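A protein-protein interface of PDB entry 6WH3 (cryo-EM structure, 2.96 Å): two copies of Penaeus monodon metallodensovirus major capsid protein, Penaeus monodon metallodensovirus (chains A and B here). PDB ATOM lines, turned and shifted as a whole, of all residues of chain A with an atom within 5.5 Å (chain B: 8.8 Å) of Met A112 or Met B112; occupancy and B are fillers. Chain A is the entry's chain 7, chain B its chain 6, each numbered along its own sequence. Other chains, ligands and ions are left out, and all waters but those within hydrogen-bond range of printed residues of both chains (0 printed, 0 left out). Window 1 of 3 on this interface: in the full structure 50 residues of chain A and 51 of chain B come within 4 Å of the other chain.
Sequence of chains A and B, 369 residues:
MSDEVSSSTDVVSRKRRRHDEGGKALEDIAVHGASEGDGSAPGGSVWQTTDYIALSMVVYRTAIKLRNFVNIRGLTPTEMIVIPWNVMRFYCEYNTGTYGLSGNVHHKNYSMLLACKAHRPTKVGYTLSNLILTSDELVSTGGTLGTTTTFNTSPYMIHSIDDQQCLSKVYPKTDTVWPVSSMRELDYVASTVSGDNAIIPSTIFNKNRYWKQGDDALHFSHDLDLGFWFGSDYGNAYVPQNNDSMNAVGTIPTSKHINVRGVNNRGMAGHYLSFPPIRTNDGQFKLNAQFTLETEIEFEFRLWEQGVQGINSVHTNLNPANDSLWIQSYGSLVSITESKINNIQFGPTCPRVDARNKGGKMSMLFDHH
OD1 of Asn B312 sits close to NZ of Lys A108. N of Trp B304 sits at hydrogen-bond distance from OD1 of Asn A109, at 3.0 Å. OG of Ser A111 sits at hydrogen-bond distance from ND2 of Asn B312 (2.9 Å). The backbone NH (N) of Trp A304 lies within hydrogen-bond range of the side-chain amide oxygen (OD1) of Asn B109 (3.0 Å).
The backbone carbonyl oxygen of Met A112 lies within hydrogen-bond range of the side-chain sulfur of Cys A116, at 3.8 Å. The backbone carbonyl oxygen (O) of Ala A115 lies within hydrogen-bond range of the indole nitrogen (NE1) of Trp A304 (2.9 Å). A ring nitrogen (ND1) of His B107 is in hydrogen-bond range of the backbone NH of Asn B109. The backbone carbonyl oxygen (O) of Leu B113 lies within hydrogen-bond range of the side-chain sulfur (SG) of Cys B116, at 3.1 Å. O of Ala B115 is in hydrogen-bond range of NE1 of Trp B304, at 2.9 Å. SG of Cys B116 sits at hydrogen-bond distance from O of Ala B118.
OD1 of Asn A109 touches CB of Leu B303 (3.3 Å). CE of Met B112 touches CE of Met A112, at 3.7 Å. Met A112 touches Cys B116 (SD to CA, 3.9 Å). Leu B303 touches Met A112. Ala A115 touches Ala B115. Cys A116 touches Met B112. OG1 of Thr B62 touches CD1 of Leu A303, 3.3 Å away. OD1 of Asn B109 touches CB of Leu A303 (3.3 Å). Leu A303 touches Met B112. Trp A304 touches Lys B108 (CZ3 to CE, 3.5 Å).
Printed residues of chain B within 4 Å of Lys A108: Trp B304 and Asn B312. Ser A111 touches one residue of chain B. Ala A115 touches just these residues of chain B: Met B112 (3.8 Å) and Ala B115 (3.6 Å). Printed residues of chain B within 4 Å of Trp A304: Lys B108 (3.5 Å) and Asn B109 (3.0 Å). Of the printed residues of chain A, Asn B109 touches Leu A303 and Trp A304. Met B112 touches just these residues of chain A: Met A112 (3.7 Å), Ala A115 (3.8 Å), Cys A116 (3.9 Å) and Leu A303 (3.2 Å). Printed residues of chain A within 4 Å of Cys B116: Met A112. Of the printed residues of chain A, Trp B304 touches Lys A108 (3.5 Å) and Asn A109 (3.0 Å). The nearest residue of chain B that does not touch Met A112 is Trp B304 (4.3 Å). The nearest residue of chain A that does not touch Met B112 is Trp A304 (4.3 Å).
Hydrophobic or aromatic side chains of chain B that line the printed part of chain A: Met B112, Ala B115, Leu B303 and Trp B304. Hydrophobic or aromatic side chains of chain A within 4 Å of the printed part of chain B: Met A112, Ala A115, Leu A303 and Trp A304. Among the printed residues, 17 pairs touch across the chains.
Asn A109 touches Trp B304, and with the chains exchanged Trp A304 touches Asn B109. Met A112 touches its own counterpart, Met B112. Met A112 touches Leu B303, and with the chains exchanged Leu A303 touches Met B112. Ala A115 touches its own counterpart, Ala B115. 12 positions are printed for both chains. Of the 17 pairs that touch across the chains among the printed residues, 14 have their exchanged pair printed and touching as well.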
ATOM      1  N   LYS A 108      31.710  -4.169  -2.365  1.00  0.00           N
ATOM      2  CA  LYS A 108      30.371  -4.737  -2.389  1.00  0.00           C
ATOM      3  C   LYS A 108      30.075  -5.612  -1.185  1.00  0.00           C
ATOM      4  O   LYS A 108      28.902  -5.814  -0.868  1.00  0.00           O
ATOM      5  CB  LYS A 108      30.139  -5.526  -3.670  1.00  0.00           C
ATOM      6  CG  LYS A 108      30.033  -4.655  -4.884  1.00  0.00           C
ATOM      7  CD  LYS A 108      29.707  -5.457  -6.101  1.00  0.00           C
ATOM      8  CE  LYS A 108      28.300  -5.984  -6.016  1.00  0.00           C
ATOM      9  NZ  LYS A 108      27.287  -4.908  -6.056  1.00  0.00           N
ATOM     10  N   ASN A 109      31.095  -6.147  -0.513  1.00  0.00           N
ATOM     11  CA  ASN A 109      30.830  -6.804   0.760  1.00  0.00           C
ATOM     12  C   ASN A 109      30.288  -5.828   1.776  1.00  0.00           C
ATOM     13  O   ASN A 109      29.526  -6.219   2.663  1.00  0.00           O
ATOM     14  CB  ASN A 109      32.080  -7.468   1.320  1.00  0.00           C
ATOM     15  CG  ASN A 109      32.415  -8.735   0.618  1.00  0.00           C
ATOM     16  OD1 ASN A 109      31.562  -9.348  -0.007  1.00  0.00           O
ATOM     17  ND2 ASN A 109      33.652  -9.166   0.747  1.00  0.00           N
ATOM     18  N   TYR A 110      30.668  -4.563   1.683  1.00  0.00           N
ATOM     19  CA  TYR A 110      30.136  -3.617   2.641  1.00  0.00           C
ATOM     20  C   TYR A 110      28.721  -3.196   2.290  1.00  0.00           C
ATOM     21  O   TYR A 110      27.917  -2.942   3.188  1.00  0.00           O
ATOM     22  CB  TYR A 110      31.019  -2.386   2.746  1.00  0.00           C
ATOM     23  CG  TYR A 110      30.426  -1.425   3.721  1.00  0.00           C
ATOM     24  CD1 TYR A 110      30.514  -1.674   5.077  1.00  0.00           C
ATOM     25  CD2 TYR A 110      29.739  -0.303   3.296  1.00  0.00           C
ATOM     26  CE1 TYR A 110      29.963  -0.835   5.981  1.00  0.00           C
ATOM     27  CE2 TYR A 110      29.180   0.549   4.199  1.00  0.00           C
ATOM     28  CZ  TYR A 110      29.297   0.269   5.542  1.00  0.00           C
ATOM     29  OH  TYR A 110      28.755   1.101   6.473  1.00  0.00           O
ATOM     30  N   SER A 111      28.407  -3.101   1.002  1.00  0.00           N
ATOM     31  CA  SER A 111      27.062  -2.715   0.605  1.00  0.00           C
ATOM     32  C   SER A 111      26.027  -3.690   1.137  1.00  0.00           C
ATOM     33  O   SER A 111      24.904  -3.289   1.452  1.00  0.00           O
ATOM     34  CB  SER A 111      26.971  -2.624  -0.914  1.00  0.00           C
ATOM     35  OG  SER A 111      27.814  -1.599  -1.404  1.00  0.00           O
ATOM     36  N   MET A 112      26.373  -4.971   1.228  1.00  0.00           N
ATOM     37  CA  MET A 112      25.440  -5.932   1.791  1.00  0.00           C
ATOM     38  C   MET A 112      25.478  -5.986   3.310  1.00  0.00           C
ATOM     39  O   MET A 112      24.535  -6.493   3.919  1.00  0.00           O
ATOM     40  CB  MET A 112      25.707  -7.323   1.264  1.00  0.00           C
ATOM     41  CG  MET A 112      26.996  -7.863   1.739  1.00  0.00           C
ATOM     42  SD  MET A 112      26.969  -9.583   1.351  1.00  0.00           S
ATOM     43  CE  MET A 112      25.894 -10.132   2.674  1.00  0.00           C
ATOM     44  N   LEU A 113      26.552  -5.522   3.947  1.00  0.00           N
ATOM     45  CA  LEU A 113      26.515  -5.418   5.399  1.00  0.00           C
ATOM     46  C   LEU A 113      25.394  -4.507   5.856  1.00  0.00           C
ATOM     47  O   LEU A 113      24.983  -4.574   7.017  1.00  0.00           O
ATOM     48  CB  LEU A 113      27.841  -4.909   5.943  1.00  0.00           C
ATOM     49  CG  LEU A 113      29.044  -5.823   5.788  1.00  0.00           C
ATOM     50  CD1 LEU A 113      30.260  -5.086   6.249  1.00  0.00           C
ATOM     51  CD2 LEU A 113      28.857  -7.076   6.591  1.00  0.00           C
ATOM     52  N   LEU A 114      24.905  -3.654   4.971  1.00  0.00           N
ATOM     53  CA  LEU A 114      23.713  -2.872   5.215  1.00  0.00           C
ATOM     54  C   LEU A 114      22.440  -3.651   4.924  1.00  0.00           C
ATOM     55  O   LEU A 114      21.357  -3.206   5.313  1.00  0.00           O
ATOM     56  CB  LEU A 114      23.755  -1.598   4.371  1.00  0.00           C
ATOM     57  CG  LEU A 114      24.538  -0.421   4.951  1.00  0.00           C
ATOM     58  CD1 LEU A 114      26.002  -0.741   5.084  1.00  0.00           C
ATOM     59  CD2 LEU A 114      24.357   0.793   4.068  1.00  0.00           C
ATOM     60  N   ALA A 115      22.545  -4.793   4.245  1.00  0.00           N
ATOM     61  CA  ALA A 115      21.388  -5.654   4.041  1.00  0.00           C
ATOM     62  C   ALA A 115      21.099  -6.507   5.268  1.00  0.00           C
ATOM     63  O   ALA A 115      19.934  -6.706   5.623  1.00  0.00           O
ATOM     64  CB  ALA A 115      21.600  -6.539   2.815  1.00  0.00           C
ATOM     65  N   CYS A 116      22.134  -7.037   5.911  1.00  0.00           N
ATOM     66  CA  CYS A 116      21.949  -7.731   7.174  1.00  0.00           C
ATOM     67  C   CYS A 116      21.665  -6.720   8.277  1.00  0.00           C
ATOM     68  O   CYS A 116      21.949  -5.529   8.142  1.00  0.00           O
ATOM     69  CB  CYS A 116      23.176  -8.570   7.511  1.00  0.00           C
ATOM     70  SG  CYS A 116      24.703  -7.654   7.525  1.00  0.00           S
ATOM     71  N   PHE A 301      28.999  -9.886  10.926  1.00  0.00           N
ATOM     72  CA  PHE A 301      27.636  -9.449  10.690  1.00  0.00           C
ATOM     73  C   PHE A 301      26.682 -10.522  11.178  1.00  0.00           C
ATOM     74  O   PHE A 301      27.074 -11.645  11.494  1.00  0.00           O
ATOM     75  CB  PHE A 301      27.394  -9.097   9.221  1.00  0.00           C
ATOM     76  CG  PHE A 301      27.565 -10.236   8.269  1.00  0.00           C
ATOM     77  CD1 PHE A 301      28.797 -10.521   7.723  1.00  0.00           C
ATOM     78  CD2 PHE A 301      26.488 -11.019   7.913  1.00  0.00           C
ATOM     79  CE1 PHE A 301      28.947 -11.561   6.847  1.00  0.00           C
ATOM     80  CE2 PHE A 301      26.635 -12.055   7.033  1.00  0.00           C
ATOM     81  CZ  PHE A 301      27.867 -12.323   6.495  1.00  0.00           C
ATOM     82  N   LEU A 303      22.290 -11.809  11.117  1.00  0.00           N
ATOM     83  CA  LEU A 303      21.148 -11.800  10.224  1.00  0.00           C
ATOM     84  C   LEU A 303      19.849 -11.567  10.984  1.00  0.00           C
ATOM     85  O   LEU A 303      19.820 -11.365  12.198  1.00  0.00           O
ATOM     86  CB  LEU A 303      21.069 -13.099   9.427  1.00  0.00           C
ATOM     87  CG  LEU A 303      22.302 -13.405   8.586  1.00  0.00           C
ATOM     88  CD1 LEU A 303      22.113 -14.662   7.760  1.00  0.00           C
ATOM     89  CD2 LEU A 303      22.711 -12.234   7.769  1.00  0.00           C
ATOM     90  N   TRP A 304      18.760 -11.583  10.232  1.00  0.00           N
ATOM     91  CA  TRP A 304      17.440 -11.176  10.677  1.00  0.00           C
ATOM     92  C   TRP A 304      16.783 -12.244  11.545  1.00  0.00           C
ATOM     93  O   TRP A 304      17.172 -13.412  11.546  1.00  0.00           O
ATOM     94  CB  TRP A 304      16.578 -10.854   9.469  1.00  0.00           C
ATOM     95  CG  TRP A 304      17.145  -9.723   8.710  1.00  0.00           C
ATOM     96  CD1 TRP A 304      17.952  -9.803   7.624  1.00  0.00           C
ATOM     97  CD2 TRP A 304      16.994  -8.335   8.997  1.00  0.00           C
ATOM     98  NE1 TRP A 304      18.294  -8.551   7.197  1.00  0.00           N
ATOM     99  CE2 TRP A 304      17.717  -7.629   8.028  1.00  0.00           C
ATOM    100  CE3 TRP A 304      16.307  -7.619   9.974  1.00  0.00           C
ATOM    101  CZ2 TRP A 304      17.776  -6.248   8.006  1.00  0.00           C
ATOM    102  CZ3 TRP A 304      16.365  -6.250   9.950  1.00  0.00           C
ATOM    103  CH2 TRP A 304      17.094  -5.577   8.974  1.00  0.00           C
ATOM    104  N   TYR B  60      28.802 -19.179   3.636  1.00  0.00           N
ATOM    105  CA  TYR B  60      28.041 -18.836   4.820  1.00  0.00           C
ATOM    106  C   TYR B  60      26.688 -19.512   4.731  1.00  0.00           C
ATOM    107  O   TYR B  60      26.126 -19.664   3.649  1.00  0.00           O
ATOM    108  CB  TYR B  60      27.856 -17.334   4.938  1.00  0.00           C
ATOM    109  CG  TYR B  60      29.133 -16.565   5.017  1.00  0.00           C
ATOM    110  CD1 TYR B  60      29.764 -16.354   6.221  1.00  0.00           C
ATOM    111  CD2 TYR B  60      29.700 -16.038   3.880  1.00  0.00           C
ATOM    112  CE1 TYR B  60      30.927 -15.646   6.288  1.00  0.00           C
ATOM    113  CE2 TYR B  60      30.857 -15.336   3.938  1.00  0.00           C
ATOM    114  CZ  TYR B  60      31.468 -15.137   5.140  1.00  0.00           C
ATOM    115  OH  TYR B  60      32.639 -14.425   5.189  1.00  0.00           O
ATOM    116  N   THR B  62      22.788 -20.012   6.269  1.00  0.00           N
ATOM    117  CA  THR B  62      21.672 -19.486   7.042  1.00  0.00           C
ATOM    118  C   THR B  62      20.433 -20.346   6.853  1.00  0.00           C
ATOM    119  O   THR B  62      20.500 -21.402   6.223  1.00  0.00           O
ATOM    120  CB  THR B  62      21.364 -18.045   6.650  1.00  0.00           C
ATOM    121  OG1 THR B  62      20.397 -17.507   7.556  1.00  0.00           O
ATOM    122  CG2 THR B  62      20.808 -17.976   5.247  1.00  0.00           C
ATOM    123  N   ILE B  64      15.732 -20.133   6.968  1.00  0.00           N
ATOM    124  CA  ILE B  64      14.481 -19.412   7.153  1.00  0.00           C
ATOM    125  C   ILE B  64      13.476 -20.376   7.752  1.00  0.00           C
ATOM    126  O   ILE B  64      13.105 -21.364   7.112  1.00  0.00           O
ATOM    127  CB  ILE B  64      13.942 -18.834   5.839  1.00  0.00           C
ATOM    128  CG1 ILE B  64      14.873 -17.753   5.313  1.00  0.00           C
ATOM    129  CG2 ILE B  64      12.554 -18.285   6.043  1.00  0.00           C
ATOM    130  CD1 ILE B  64      14.542 -17.323   3.930  1.00  0.00           C
ATOM    131  N   HIS B 106       8.220 -12.027   1.734  1.00  0.00           N
ATOM    132  CA  HIS B 106       9.448 -12.794   1.862  1.00  0.00           C
ATOM    133  C   HIS B 106      10.116 -12.528   3.202  1.00  0.00           C
ATOM    134  O   HIS B 106      10.052 -11.426   3.747  1.00  0.00           O
ATOM    135  CB  HIS B 106      10.408 -12.431   0.737  1.00  0.00           C
ATOM    136  CG  HIS B 106       9.860 -12.687  -0.627  1.00  0.00           C
ATOM    137  ND1 HIS B 106       9.713 -13.954  -1.144  1.00  0.00           N
ATOM    138  CD2 HIS B 106       9.393 -11.838  -1.570  1.00  0.00           C
ATOM    139  CE1 HIS B 106       9.202 -13.873  -2.358  1.00  0.00           C
ATOM    140  NE2 HIS B 106       8.995 -12.600  -2.639  1.00  0.00           N
ATOM    141  N   HIS B 107      10.759 -13.555   3.737  1.00  0.00           N
ATOM    142  CA  HIS B 107      11.524 -13.395   4.959  1.00  0.00           C
ATOM    143  C   HIS B 107      12.754 -12.543   4.679  1.00  0.00           C
ATOM    144  O   HIS B 107      13.327 -12.586   3.591  1.00  0.00           O
ATOM    145  CB  HIS B 107      11.923 -14.759   5.500  1.00  0.00           C
ATOM    146  CG  HIS B 107      12.510 -14.724   6.872  1.00  0.00           C
ATOM    147  ND1 HIS B 107      13.823 -14.394   7.114  1.00  0.00           N
ATOM    148  CD2 HIS B 107      11.967 -15.009   8.077  1.00  0.00           C
ATOM    149  CE1 HIS B 107      14.061 -14.461   8.409  1.00  0.00           C
ATOM    150  NE2 HIS B 107      12.951 -14.832   9.016  1.00  0.00           N
ATOM    151  N   LYS B 108      13.158 -11.751   5.671  1.00  0.00           N
ATOM    152  CA  LYS B 108      14.218 -10.785   5.424  1.00  0.00           C
ATOM    153  C   LYS B 108      15.581 -11.430   5.257  1.00  0.00           C
ATOM    154  O   LYS B 108      16.464 -10.813   4.655  1.00  0.00           O
ATOM    155  CB  LYS B 108      14.272  -9.742   6.531  1.00  0.00           C
ATOM    156  CG  LYS B 108      13.106  -8.803   6.507  1.00  0.00           C
ATOM    157  CD  LYS B 108      13.247  -7.737   7.544  1.00  0.00           C
ATOM    158  CE  LYS B 108      14.364  -6.798   7.177  1.00  0.00           C
ATOM    159  NZ  LYS B 108      14.075  -6.021   5.952  1.00  0.00           N
ATOM    160  N   ASN B 109      15.789 -12.639   5.777  1.00  0.00           N
ATOM    161  CA  ASN B 109      17.015 -13.351   5.438  1.00  0.00           C
ATOM    162  C   ASN B 109      17.081 -13.650   3.959  1.00  0.00           C
ATOM    163  O   ASN B 109      18.172 -13.730   3.394  1.00  0.00           O
ATOM    164  CB  ASN B 109      17.145 -14.650   6.219  1.00  0.00           C
ATOM    165  CG  ASN B 109      17.545 -14.426   7.634  1.00  0.00           C
ATOM    166  OD1 ASN B 109      18.102 -13.391   7.971  1.00  0.00           O
ATOM    167  ND2 ASN B 109      17.303 -15.411   8.473  1.00  0.00           N
ATOM    168  N   TYR B 110      15.939 -13.833   3.314  1.00  0.00           N
ATOM    169  CA  TYR B 110      15.994 -14.100   1.892  1.00  0.00           C
ATOM    170  C   TYR B 110      16.221 -12.833   1.089  1.00  0.00           C
ATOM    171  O   TYR B 110      16.878 -12.878   0.047  1.00  0.00           O
ATOM    172  CB  TYR B 110      14.724 -14.782   1.412  1.00  0.00           C
ATOM    173  CG  TYR B 110      14.806 -15.016  -0.058  1.00  0.00           C
ATOM    174  CD1 TYR B 110      15.604 -16.031  -0.552  1.00  0.00           C
ATOM    175  CD2 TYR B 110      14.133 -14.206  -0.954  1.00  0.00           C
ATOM    176  CE1 TYR B 110      15.719 -16.249  -1.880  1.00  0.00           C
ATOM    177  CE2 TYR B 110      14.242 -14.419  -2.294  1.00  0.00           C
ATOM    178  CZ  TYR B 110      15.042 -15.444  -2.746  1.00  0.00           C
ATOM    179  OH  TYR B 110      15.169 -15.688  -4.079  1.00  0.00           O
ATOM    180  N   SER B 111      15.679 -11.708   1.544  1.00  0.00           N
ATOM    181  CA  SER B 111      15.874 -10.459   0.824  1.00  0.00           C
ATOM    182  C   SER B 111      17.347 -10.109   0.717  1.00  0.00           C
ATOM    183  O   SER B 111      17.771  -9.516  -0.279  1.00  0.00           O
ATOM    184  CB  SER B 111      15.110  -9.334   1.512  1.00  0.00           C
ATOM    185  OG  SER B 111      13.718  -9.577   1.468  1.00  0.00           O
ATOM    186  N   MET B 112      18.138 -10.447   1.731  1.00  0.00           N
ATOM    187  CA  MET B 112      19.567 -10.188   1.647  1.00  0.00           C
ATOM    188  C   MET B 112      20.330 -11.275   0.908  1.00  0.00           C
ATOM    189  O   MET B 112      21.460 -11.033   0.479  1.00  0.00           O
ATOM    190  CB  MET B 112      20.174 -10.040   3.023  1.00  0.00           C
ATOM    191  CG  MET B 112      20.155 -11.305   3.782  1.00  0.00           C
ATOM    192  SD  MET B 112      21.213 -11.050   5.170  1.00  0.00           S
ATOM    193  CE  MET B 112      22.787 -11.211   4.333  1.00  0.00           C
ATOM    194  N   LEU B 113      19.777 -12.479   0.778  1.00  0.00           N
ATOM    195  CA  LEU B 113      20.431 -13.463  -0.075  1.00  0.00           C
ATOM    196  C   LEU B 113      20.557 -12.960  -1.498  1.00  0.00           C
ATOM    197  O   LEU B 113      21.377 -13.475  -2.260  1.00  0.00           O
ATOM    198  CB  LEU B 113      19.675 -14.783  -0.064  1.00  0.00           C
ATOM    199  CG  LEU B 113      19.658 -15.555   1.243  1.00  0.00           C
ATOM    200  CD1 LEU B 113      18.752 -16.733   1.085  1.00  0.00           C
ATOM    201  CD2 LEU B 113      21.042 -16.006   1.604  1.00  0.00           C
ATOM    202  N   LEU B 114      19.755 -11.975  -1.868  1.00  0.00           N
ATOM    203  CA  LEU B 114      19.903 -11.275  -3.126  1.00  0.00           C
ATOM    204  C   LEU B 114      20.952 -10.176  -3.054  1.00  0.00           C
ATOM    205  O   LEU B 114      21.360  -9.661  -4.098  1.00  0.00           O
ATOM    206  CB  LEU B 114      18.556 -10.693  -3.548  1.00  0.00           C
ATOM    207  CG  LEU B 114      17.607 -11.635  -4.288  1.00  0.00           C
ATOM    208  CD1 LEU B 114      17.175 -12.783  -3.418  1.00  0.00           C
ATOM    209  CD2 LEU B 114      16.393 -10.865  -4.761  1.00  0.00           C
ATOM    210  N   ALA B 115      21.386  -9.800  -1.851  1.00  0.00           N
ATOM    211  CA  ALA B 115      22.478  -8.845  -1.711  1.00  0.00           C
ATOM    212  C   ALA B 115      23.833  -9.511  -1.903  1.00  0.00           C
ATOM    213  O   ALA B 115      24.728  -8.927  -2.521  1.00  0.00           O
ATOM    214  CB  ALA B 115      22.408  -8.160  -0.349  1.00  0.00           C
ATOM    215  N   CYS B 116      24.015 -10.711  -1.362  1.00  0.00           N
ATOM    216  CA  CYS B 116      25.223 -11.473  -1.632  1.00  0.00           C
ATOM    217  C   CYS B 116      25.178 -12.017  -3.054  1.00  0.00           C
ATOM    218  O   CYS B 116      24.117 -12.104  -3.672  1.00  0.00           O
ATOM    219  CB  CYS B 116      25.381 -12.604  -0.622  1.00  0.00           C
ATOM    220  SG  CYS B 116      23.973 -13.690  -0.520  1.00  0.00           S
ATOM    221  N   LYS B 117      26.345 -12.367  -3.590  1.00  0.00           N
ATOM    222  CA  LYS B 117      26.375 -12.652  -5.018  1.00  0.00           C
ATOM    223  C   LYS B 117      25.841 -14.028  -5.364  1.00  0.00           C
ATOM    224  O   LYS B 117      25.393 -14.234  -6.495  1.00  0.00           O
ATOM    225  CB  LYS B 117      27.779 -12.535  -5.593  1.00  0.00           C
ATOM    226  CG  LYS B 117      28.768 -13.563  -5.150  1.00  0.00           C
ATOM    227  CD  LYS B 117      30.020 -13.303  -5.937  1.00  0.00           C
ATOM    228  CE  LYS B 117      29.731 -13.518  -7.410  1.00  0.00           C
ATOM    229  NZ  LYS B 117      30.886 -13.231  -8.285  1.00  0.00           N
ATOM    230  N   ALA B 118      25.891 -14.972  -4.439  1.00  0.00           N
ATOM    231  CA  ALA B 118      25.451 -16.327  -4.704  1.00  0.00           C
ATOM    232  C   ALA B 118      24.745 -16.871  -3.481  1.00  0.00           C
ATOM    233  O   ALA B 118      25.176 -16.628  -2.354  1.00  0.00           O
ATOM    234  CB  ALA B 118      26.625 -17.233  -5.051  1.00  0.00           C
ATOM    235  N   HIS B 119      23.667 -17.607  -3.705  1.00  0.00           N
ATOM    236  CA  HIS B 119      23.021 -18.345  -2.638  1.00  0.00           C
ATOM    237  C   HIS B 119      22.577 -19.686  -3.184  1.00  0.00           C
ATOM    238  O   HIS B 119      22.321 -19.833  -4.378  1.00  0.00           O
ATOM    239  CB  HIS B 119      21.811 -17.627  -2.064  1.00  0.00           C
ATOM    240  CG  HIS B 119      20.710 -17.436  -3.049  1.00  0.00           C
ATOM    241  ND1 HIS B 119      20.746 -16.470  -4.027  1.00  0.00           N
ATOM    242  CD2 HIS B 119      19.550 -18.107  -3.225  1.00  0.00           C
ATOM    243  CE1 HIS B 119      19.647 -16.542  -4.752  1.00  0.00           C
ATOM    244  NE2 HIS B 119      18.906 -17.529  -4.289  1.00  0.00           N
ATOM    245  N   PHE B 301      25.110 -19.184   1.359  1.00  0.00           N
ATOM    246  CA  PHE B 301      25.356 -18.034   0.510  1.00  0.00           C
ATOM    247  C   PHE B 301      26.838 -17.712   0.534  1.00  0.00           C
ATOM    248  O   PHE B 301      27.603 -18.235   1.342  1.00  0.00           O
ATOM    249  CB  PHE B 301      24.504 -16.830   0.916  1.00  0.00           C
ATOM    250  CG  PHE B 301      24.771 -16.312   2.292  1.00  0.00           C
ATOM    251  CD1 PHE B 301      24.097 -16.819   3.381  1.00  0.00           C
ATOM    252  CD2 PHE B 301      25.693 -15.307   2.495  1.00  0.00           C
ATOM    253  CE1 PHE B 301      24.340 -16.337   4.638  1.00  0.00           C
ATOM    254  CE2 PHE B 301      25.931 -14.820   3.750  1.00  0.00           C
ATOM    255  CZ  PHE B 301      25.251 -15.334   4.823  1.00  0.00           C
ATOM    256  N   ARG B 302      27.236 -16.855  -0.392  1.00  0.00           N
ATOM    257  CA  ARG B 302      28.637 -16.607  -0.673  1.00  0.00           C
ATOM    258  C   ARG B 302      28.795 -15.154  -1.080  1.00  0.00           C
ATOM    259  O   ARG B 302      27.909 -14.588  -1.718  1.00  0.00           O
ATOM    260  CB  ARG B 302      29.132 -17.577  -1.750  1.00  0.00           C
ATOM    261  CG  ARG B 302      30.495 -17.290  -2.257  1.00  0.00           C
ATOM    262  CD  ARG B 302      30.967 -18.332  -3.234  1.00  0.00           C
ATOM    263  NE  ARG B 302      31.349 -19.562  -2.559  1.00  0.00           N
ATOM    264  CZ  ARG B 302      31.784 -20.643  -3.186  1.00  0.00           C
ATOM    265  NH1 ARG B 302      31.875 -20.654  -4.500  1.00  0.00           N
ATOM    266  NH2 ARG B 302      32.138 -21.710  -2.498  1.00  0.00           N
ATOM    267  N   LEU B 303      29.909 -14.547  -0.690  1.00  0.00           N
ATOM    268  CA  LEU B 303      30.031 -13.105  -0.788  1.00  0.00           C
ATOM    269  C   LEU B 303      30.880 -12.699  -1.986  1.00  0.00           C
ATOM    270  O   LEU B 303      31.344 -13.520  -2.777  1.00  0.00           O
ATOM    271  CB  LEU B 303      30.613 -12.519   0.495  1.00  0.00           C
ATOM    272  CG  LEU B 303      29.809 -12.823   1.752  1.00  0.00           C
ATOM    273  CD1 LEU B 303      30.400 -12.136   2.968  1.00  0.00           C
ATOM    274  CD2 LEU B 303      28.366 -12.522   1.565  1.00  0.00           C
ATOM    275  N   TRP B 304      31.063 -11.394  -2.115  1.00  0.00           N
ATOM    276  CA  TRP B 304      31.645 -10.751  -3.279  1.00  0.00           C
ATOM    277  C   TRP B 304      33.160 -10.906  -3.312  1.00  0.00           C
ATOM    278  O   TRP B 304      33.807 -11.208  -2.309  1.00  0.00           O
ATOM    279  CB  TRP B 304      31.249  -9.285  -3.292  1.00  0.00           C
ATOM    280  CG  TRP B 304      29.785  -9.139  -3.404  1.00  0.00           C
ATOM    281  CD1 TRP B 304      28.911  -8.962  -2.384  1.00  0.00           C
ATOM    282  CD2 TRP B 304      29.006  -9.203  -4.596  1.00  0.00           C
ATOM    283  NE1 TRP B 304      27.634  -8.886  -2.865  1.00  0.00           N
ATOM    284  CE2 TRP B 304      27.667  -9.032  -4.225  1.00  0.00           C
ATOM    285  CE3 TRP B 304      29.311  -9.377  -5.943  1.00  0.00           C
ATOM    286  CZ2 TRP B 304      26.635  -9.032  -5.147  1.00  0.00           C
ATOM    287  CZ3 TRP B 304      28.287  -9.375  -6.855  1.00  0.00           C
ATOM    288  CH2 TRP B 304      26.966  -9.205  -6.456  1.00  0.00           C
ATOM    289  N   ASN B 312      31.986  -1.432  -5.915  1.00  0.00           N
ATOM    290  CA  ASN B 312      30.702  -1.281  -6.596  1.00  0.00           C
ATOM    291  C   ASN B 312      30.855  -0.658  -7.975  1.00  0.00           C
ATOM    292  O   ASN B 312      30.270  -1.136  -8.952  1.00  0.00           O
ATOM    293  CB  ASN B 312      29.749  -0.438  -5.754  1.00  0.00           C
ATOM    294  CG  ASN B 312      29.207  -1.181  -4.564  1.00  0.00           C
ATOM    295  OD1 ASN B 312      28.308  -2.005  -4.695  1.00  0.00           O
ATOM    296  ND2 ASN B 312      29.737  -0.886  -3.390  1.00  0.00           N
